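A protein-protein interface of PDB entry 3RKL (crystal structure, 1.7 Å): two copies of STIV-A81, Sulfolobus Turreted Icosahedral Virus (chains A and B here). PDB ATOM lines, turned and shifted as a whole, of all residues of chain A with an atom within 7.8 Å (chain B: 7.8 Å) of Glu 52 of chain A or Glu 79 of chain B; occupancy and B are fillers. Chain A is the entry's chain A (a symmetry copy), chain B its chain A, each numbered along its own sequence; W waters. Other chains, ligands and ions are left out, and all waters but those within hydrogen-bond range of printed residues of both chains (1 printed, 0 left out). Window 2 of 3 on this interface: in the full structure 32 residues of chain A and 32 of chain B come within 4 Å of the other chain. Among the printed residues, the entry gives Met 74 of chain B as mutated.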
ATOM      1  N   ILE A  43      14.905  26.309   1.814  1.00  0.00           N
ATOM      2  CA  ILE A  43      14.265  26.518   0.514  1.00  0.00           C
ATOM      3  C   ILE A  43      12.842  25.954   0.540  1.00  0.00           C
ATOM      4  O   ILE A  43      11.899  26.606   0.092  1.00  0.00           O
ATOM      5  CB  ILE A  43      15.107  25.924  -0.617  1.00  0.00           C
ATOM      6  CG1 ILE A  43      16.387  26.736  -0.796  1.00  0.00           C
ATOM      7  CG2 ILE A  43      14.303  25.871  -1.918  1.00  0.00           C
ATOM      8  CD1 ILE A  43      17.409  26.074  -1.700  1.00  0.00           C
ATOM      9  N   LEU A  46      10.642  28.296   2.710  1.00  0.00           N
ATOM     10  CA  LEU A  46      10.403  29.584   2.040  1.00  0.00           C
ATOM     11  C   LEU A  46       9.432  29.418   0.880  1.00  0.00           C
ATOM     12  O   LEU A  46       8.665  30.332   0.558  1.00  0.00           O
ATOM     13  CB  LEU A  46      11.701  30.210   1.539  1.00  0.00           C
ATOM     14  CG  LEU A  46      12.606  30.824   2.602  1.00  0.00           C
ATOM     15  CD1 LEU A  46      13.946  31.179   1.992  1.00  0.00           C
ATOM     16  CD2 LEU A  46      11.953  32.052   3.214  1.00  0.00           C
ATOM     17  N   SER A  47       9.453  28.243   0.263  1.00  0.00           N
ATOM     18  CA  SER A  47       8.575  27.959  -0.877  1.00  0.00           C
ATOM     19  C   SER A  47       7.078  27.977  -0.545  1.00  0.00           C
ATOM     20  O   SER A  47       6.248  28.133  -1.445  1.00  0.00           O
ATOM     21  CB  SER A  47       8.959  26.618  -1.520  1.00  0.00           C
ATOM     22  OG  SER A  47      10.236  26.707  -2.117  1.00  0.00           O
ATOM     23  N   TYR A  49       5.675  30.372   0.960  1.00  0.00           N
ATOM     24  CA  TYR A  49       5.295  31.785   0.847  1.00  0.00           C
ATOM     25  C   TYR A  49       5.825  32.482  -0.394  1.00  0.00           C
ATOM     26  O   TYR A  49       5.252  33.478  -0.837  1.00  0.00           O
ATOM     27  CB  TYR A  49       5.746  32.542   2.092  1.00  0.00           C
ATOM     28  CG  TYR A  49       5.030  32.060   3.332  1.00  0.00           C
ATOM     29  CD1 TYR A  49       3.701  32.392   3.553  1.00  0.00           C
ATOM     30  CD2 TYR A  49       5.669  31.250   4.265  1.00  0.00           C
ATOM     31  CE1 TYR A  49       3.029  31.946   4.670  1.00  0.00           C
ATOM     32  CE2 TYR A  49       5.001  30.795   5.393  1.00  0.00           C
ATOM     33  CZ  TYR A  49       3.678  31.152   5.584  1.00  0.00           C
ATOM     34  OH  TYR A  49       2.997  30.717   6.677  1.00  0.00           O
ATOM     35  N   GLU A  50       6.905  31.964  -0.963  1.00  0.00           N
ATOM     36  CA  GLU A  50       7.544  32.627  -2.094  1.00  0.00           C
ATOM     37  C   GLU A  50       7.346  31.846  -3.377  1.00  0.00           C
ATOM     38  O   GLU A  50       7.720  30.685  -3.462  1.00  0.00           O
ATOM     39  CB  GLU A  50       9.032  32.796  -1.824  1.00  0.00           C
ATOM     40  CG  GLU A  50       9.319  33.531  -0.531  1.00  0.00           C
ATOM     41  CD  GLU A  50      10.712  34.122  -0.477  1.00  0.00           C
ATOM     42  OE1 GLU A  50      11.529  33.829  -1.375  1.00  0.00           O
ATOM     43  OE2 GLU A  50      10.985  34.894   0.467  1.00  0.00           O
ATOM     44  N   GLU A  51       6.752  32.493  -4.374  1.00  0.00           N
ATOM     45  CA  GLU A  51       6.657  31.903  -5.704  1.00  0.00           C
ATOM     46  C   GLU A  51       8.054  31.563  -6.215  1.00  0.00           C
ATOM     47  O   GLU A  51       8.287  30.454  -6.697  1.00  0.00           O
ATOM     48  CB  GLU A  51       5.940  32.845  -6.670  1.00  0.00           C
ATOM     49  CG  GLU A  51       4.446  32.982  -6.380  1.00  0.00           C
ATOM     50  CD  GLU A  51       3.676  33.631  -7.516  1.00  0.00           C
ATOM     51  OE1 GLU A  51       3.812  33.172  -8.669  1.00  0.00           O
ATOM     52  OE2 GLU A  51       2.923  34.593  -7.253  1.00  0.00           O
ATOM     53  N   GLU A  52       8.976  32.515  -6.070  1.00  0.00           N
ATOM     54  CA  GLU A  52      10.384  32.336  -6.445  1.00  0.00           C
ATOM     55  C   GLU A  52      11.286  32.513  -5.237  1.00  0.00           C
ATOM     56  O   GLU A  52      11.426  33.622  -4.724  1.00  0.00           O
ATOM     57  CB  GLU A  52      10.802  33.374  -7.497  1.00  0.00           C
ATOM     58  CG  GLU A  52      10.221  33.165  -8.890  1.00  0.00           C
ATOM     59  CD  GLU A  52      11.058  32.231  -9.755  1.00  0.00           C
ATOM     60  OE1 GLU A  52      11.302  32.566 -10.934  1.00  0.00           O
ATOM     61  OE2 GLU A  52      11.472  31.164  -9.256  1.00  0.00           O
ATOM     62  N   VAL A  53      11.907  31.429  -4.785  1.00  0.00           N
ATOM     63  CA  VAL A  53      12.935  31.525  -3.759  1.00  0.00           C
ATOM     64  C   VAL A  53      14.233  32.051  -4.396  1.00  0.00           C
ATOM     65  O   VAL A  53      14.582  31.670  -5.519  1.00  0.00           O
ATOM     66  CB  VAL A  53      13.137  30.177  -3.049  1.00  0.00           C
ATOM     67  CG1 VAL A  53      14.311  30.242  -2.073  1.00  0.00           C
ATOM     68  CG2 VAL A  53      11.861  29.787  -2.322  1.00  0.00           C
ATOM     69  N   ASP A  54      14.917  32.952  -3.693  1.00  0.00           N
ATOM     70  CA  ASP A  54      16.132  33.597  -4.235  1.00  0.00           C
ATOM     71  C   ASP A  54      17.121  32.593  -4.823  1.00  0.00           C
ATOM     72  O   ASP A  54      17.470  31.592  -4.178  1.00  0.00           O
ATOM     73  CB  ASP A  54      16.843  34.421  -3.163  1.00  0.00           C
ATOM     74  CG  ASP A  54      16.151  35.748  -2.876  1.00  0.00           C
ATOM     75  OD1 ASP A  54      15.336  36.212  -3.706  1.00  0.00           O
ATOM     76  OD2 ASP A  54      16.434  36.328  -1.807  1.00  0.00           O
ATOM     77  N   THR A  55      17.578  32.878  -6.044  1.00  0.00           N
ATOM     78  CA  THR A  55      18.546  32.034  -6.753  1.00  0.00           C
ATOM     79  C   THR A  55      19.822  31.829  -5.957  1.00  0.00           C
ATOM     80  O   THR A  55      20.470  30.786  -6.078  1.00  0.00           O
ATOM     81  CB  THR A  55      18.929  32.642  -8.123  1.00  0.00           C
ATOM     82  OG1 THR A  55      17.753  32.782  -8.926  1.00  0.00           O
ATOM     83  CG2 THR A  55      19.927  31.746  -8.843  1.00  0.00           C
ATOM     84  N   TYR A  58      19.722  28.581  -3.980  1.00  0.00           N
ATOM     85  CA  TYR A  58      19.966  27.394  -4.820  1.00  0.00           C
ATOM     86  C   TYR A  58      21.449  27.270  -5.205  1.00  0.00           C
ATOM     87  O   TYR A  58      22.004  26.157  -5.247  1.00  0.00           O
ATOM     88  CB  TYR A  58      19.107  27.398  -6.088  1.00  0.00           C
ATOM     89  CG  TYR A  58      17.617  27.249  -5.848  1.00  0.00           C
ATOM     90  CD1 TYR A  58      17.010  26.009  -5.845  1.00  0.00           C
ATOM     91  CD2 TYR A  58      16.813  28.370  -5.652  1.00  0.00           C
ATOM     92  CE1 TYR A  58      15.635  25.881  -5.621  1.00  0.00           C
ATOM     93  CE2 TYR A  58      15.441  28.250  -5.434  1.00  0.00           C
ATOM     94  CZ  TYR A  58      14.862  27.006  -5.422  1.00  0.00           C
ATOM     95  OH  TYR A  58      13.506  26.889  -5.199  1.00  0.00           O
ATOM     96  N   LEU B  25      13.420  15.888  -6.297  1.00  0.00           N
ATOM     97  CA  LEU B  25      14.683  16.557  -5.957  1.00  0.00           C
ATOM     98  C   LEU B  25      14.680  17.167  -4.557  1.00  0.00           C
ATOM     99  O   LEU B  25      15.628  16.963  -3.796  1.00  0.00           O
ATOM    100  CB  LEU B  25      15.087  17.598  -7.001  1.00  0.00           C
ATOM    101  CG  LEU B  25      15.484  17.060  -8.377  1.00  0.00           C
ATOM    102  CD1 LEU B  25      15.830  18.191  -9.342  1.00  0.00           C
ATOM    103  CD2 LEU B  25      16.658  16.079  -8.247  1.00  0.00           C
ATOM    104  N   SER B  73      22.647  20.108  -8.569  1.00  0.00           N
ATOM    105  CA  SER B  73      22.851  20.702  -9.887  1.00  0.00           C
ATOM    106  C   SER B  73      21.548  20.684 -10.663  1.00  0.00           C
ATOM    107  O   SER B  73      21.162  21.683 -11.274  1.00  0.00           O
ATOM    108  CB  SER B  73      23.928  19.956 -10.670  1.00  0.00           C
ATOM    109  OG  SER B  73      24.209  20.636 -11.882  1.00  0.00           O
ATOM    110  N   MET B  74      20.885  19.533 -10.642  1.00  0.00           N
ATOM    111  CA  MET B  74      19.585  19.379 -11.319  1.00  0.00           C
ATOM    112  C   MET B  74      18.557  20.370 -10.757  1.00  0.00           C
ATOM    113  O   MET B  74      17.720  20.902 -11.485  1.00  0.00           O
ATOM    114  CB  MET B  74      19.054  17.953 -11.149  1.00  0.00           C
ATOM    115  CG  MET B  74      19.884  16.860 -11.802  1.00  0.00           C
ATOM    116  SD  MET B  74      19.334  15.054 -11.205  1.00  0.00           S
ATOM    117  CE  MET B  74      17.423  15.190 -11.601  1.00  0.00           C
ATOM    118  N   PHE B  75      18.619  20.587  -9.444  1.00  0.00           N
ATOM    119  CA  PHE B  75      17.687  21.457  -8.719  1.00  0.00           C
ATOM    120  C   PHE B  75      17.814  22.909  -9.185  1.00  0.00           C
ATOM    121  O   PHE B  75      16.813  23.576  -9.415  1.00  0.00           O
ATOM    122  CB  PHE B  75      17.962  21.287  -7.214  1.00  0.00           C
ATOM    123  CG  PHE B  75      16.836  21.696  -6.284  1.00  0.00           C
ATOM    124  CD1 PHE B  75      15.529  21.294  -6.483  1.00  0.00           C
ATOM    125  CD2 PHE B  75      17.140  22.395  -5.123  1.00  0.00           C
ATOM    126  CE1 PHE B  75      14.537  21.636  -5.572  1.00  0.00           C
ATOM    127  CE2 PHE B  75      16.167  22.731  -4.213  1.00  0.00           C
ATOM    128  CZ  PHE B  75      14.858  22.360  -4.440  1.00  0.00           C
ATOM    129  N   ILE B  76      19.041  23.397  -9.348  1.00  0.00           N
ATOM    130  CA  ILE B  76      19.230  24.793  -9.745  1.00  0.00           C
ATOM    131  C   ILE B  76      18.959  25.012 -11.229  1.00  0.00           C
ATOM    132  O   ILE B  76      18.389  26.036 -11.610  1.00  0.00           O
ATOM    133  CB  ILE B  76      20.614  25.371  -9.324  1.00  0.00           C
ATOM    134  CG1 ILE B  76      20.781  26.783  -9.903  1.00  0.00           C
ATOM    135  CG2 ILE B  76      21.755  24.498  -9.764  1.00  0.00           C
ATOM    136  CD1 ILE B  76      21.890  27.555  -9.253  1.00  0.00           C
ATOM    137  N   ASP B  77      19.365  24.058 -12.063  1.00  0.00           N
ATOM    138  CA  ASP B  77      19.055  24.101 -13.488  1.00  0.00           C
ATOM    139  C   ASP B  77      17.545  24.188 -13.686  1.00  0.00           C
ATOM    140  O   ASP B  77      17.057  24.984 -14.488  1.00  0.00           O
ATOM    141  CB  ASP B  77      19.572  22.845 -14.190  1.00  0.00           C
ATOM    142  CG  ASP B  77      21.086  22.815 -14.325  1.00  0.00           C
ATOM    143  OD1 ASP B  77      21.780  23.741 -13.850  1.00  0.00           O
ATOM    144  OD2 ASP B  77      21.588  21.829 -14.901  1.00  0.00           O
ATOM    145  N   SER B  78      16.822  23.349 -12.949  1.00  0.00           N
ATOM    146  CA  SER B  78      15.361  23.313 -13.021  1.00  0.00           C
ATOM    147  C   SER B  78      14.723  24.614 -12.552  1.00  0.00           C
ATOM    148  O   SER B  78      13.737  25.072 -13.131  1.00  0.00           O
ATOM    149  CB  SER B  78      14.818  22.161 -12.176  1.00  0.00           C
ATOM    150  OG  SER B  78      13.424  22.007 -12.386  1.00  0.00           O
ATOM    151  N   GLU B  79      15.268  25.186 -11.485  1.00  0.00           N
ATOM    152  CA  GLU B  79      14.767  26.445 -10.948  1.00  0.00           C
ATOM    153  C   GLU B  79      14.974  27.586 -11.950  1.00  0.00           C
ATOM    154  O   GLU B  79      14.073  28.405 -12.153  1.00  0.00           O
ATOM    155  CB  GLU B  79      15.438  26.758  -9.601  1.00  0.00           C
ATOM    156  CG  GLU B  79      15.042  28.094  -8.995  1.00  0.00           C
ATOM    157  CD  GLU B  79      13.578  28.166  -8.578  1.00  0.00           C
ATOM    158  OE1 GLU B  79      12.915  27.108  -8.482  1.00  0.00           O
ATOM    159  OE2 GLU B  79      13.094  29.295  -8.339  1.00  0.00           O
ATOM    160  N   ASN B  80      16.147  27.632 -12.586  1.00  0.00           N
ATOM    161  CA  ASN B  80      16.415  28.678 -13.581  1.00  0.00           C
ATOM    162  C   ASN B  80      15.536  28.559 -14.829  1.00  0.00           C
ATOM    163  O   ASN B  80      15.189  29.573 -15.454  1.00  0.00           O
ATOM    164  CB  ASN B  80      17.899  28.702 -13.950  1.00  0.00           C
ATOM    165  CG  ASN B  80      18.765  29.241 -12.828  1.00  0.00           C
ATOM    166  OD1 ASN B  80      18.268  29.855 -11.879  1.00  0.00           O
ATOM    167  ND2 ASN B  80      20.062  29.008 -12.923  1.00  0.00           N
ATOM    168  N   LYS B  81      15.162  27.329 -15.174  1.00  0.00           N
ATOM    169  CA  LYS B  81      14.228  27.079 -16.269  1.00  0.00           C
ATOM    170  C   LYS B  81      12.832  27.583 -15.918  1.00  0.00           C
ATOM    171  O   LYS B  81      12.116  28.078 -16.789  1.00  0.00           O
ATOM    172  CB  LYS B  81      14.168  25.587 -16.614  1.00  0.00           C
ATOM    173  CG  LYS B  81      15.348  25.093 -17.439  1.00  0.00           C
ATOM    174  CD  LYS B  81      15.322  23.582 -17.630  1.00  0.00           C
ATOM    175  CE  LYS B  81      16.660  23.063 -18.142  1.00  0.00           C
ATOM    176  NZ  LYS B  81      16.677  21.582 -18.281  1.00  0.00           N
HETATM  177  O   HOH W   1      11.660  28.795  -6.032  1.00  0.00           O
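The side-chain carboxylate (OE2) of Glu 52 of chain A sits close to the side-chain carboxylate (OE2) of Glu 79 of chain B (2.6 Å).
The side-chain carboxylate of Glu 79 of chain B is in hydrogen-bond range of the side-chain hydroxyl of Tyr 58 of chain A (3.3 Å).
Among the printed residues, pairs that only touch across the chains: Val 53 of chain A with Glu 79 of chain B (3.98 Å), Thr 55 of chain A with Asn 80 of chain B (3.9 Å) and Tyr 58 of chain A with Phe 75 of chain B (3.5 Å).
Glu 52 of chain A touches one residue of chain B.
Of the printed residues of chain A, Glu 79 of chain B touches Glu 52, Val 53 and Tyr 58.
Of the printed residues of chain B, Thr 55 of chain A touches Asn 80.
Of the printed residues of chain B, Val 53 of chain A touches Glu 79 (3.98 Å).
Printed residues of chain A within 4 Å of Phe 75 of chain B: Tyr 58 (3.5 Å).
Printed residues of chain A within 4 Å of Asn 80 of chain B: Thr 55.
The nearest residue of chain B that does not touch Glu 52 of chain A is Asn 80 of chain B (6.7 Å).
Hydrophobic or aromatic side chains of chain B that line the printed part of chain A: Phe 75.
Hydrophobic or aromatic side chains of chain A within 4 Å of the printed part of chain B: Tyr 58.
No position is printed for both chains.
Water W1 lies within hydrogen-bond range of OE2 of Glu 79 of chain B (2.8 Å), OH of Tyr 58 of chain A (2.8 Å) and N of Val 53 of chain A (2.9 Å).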
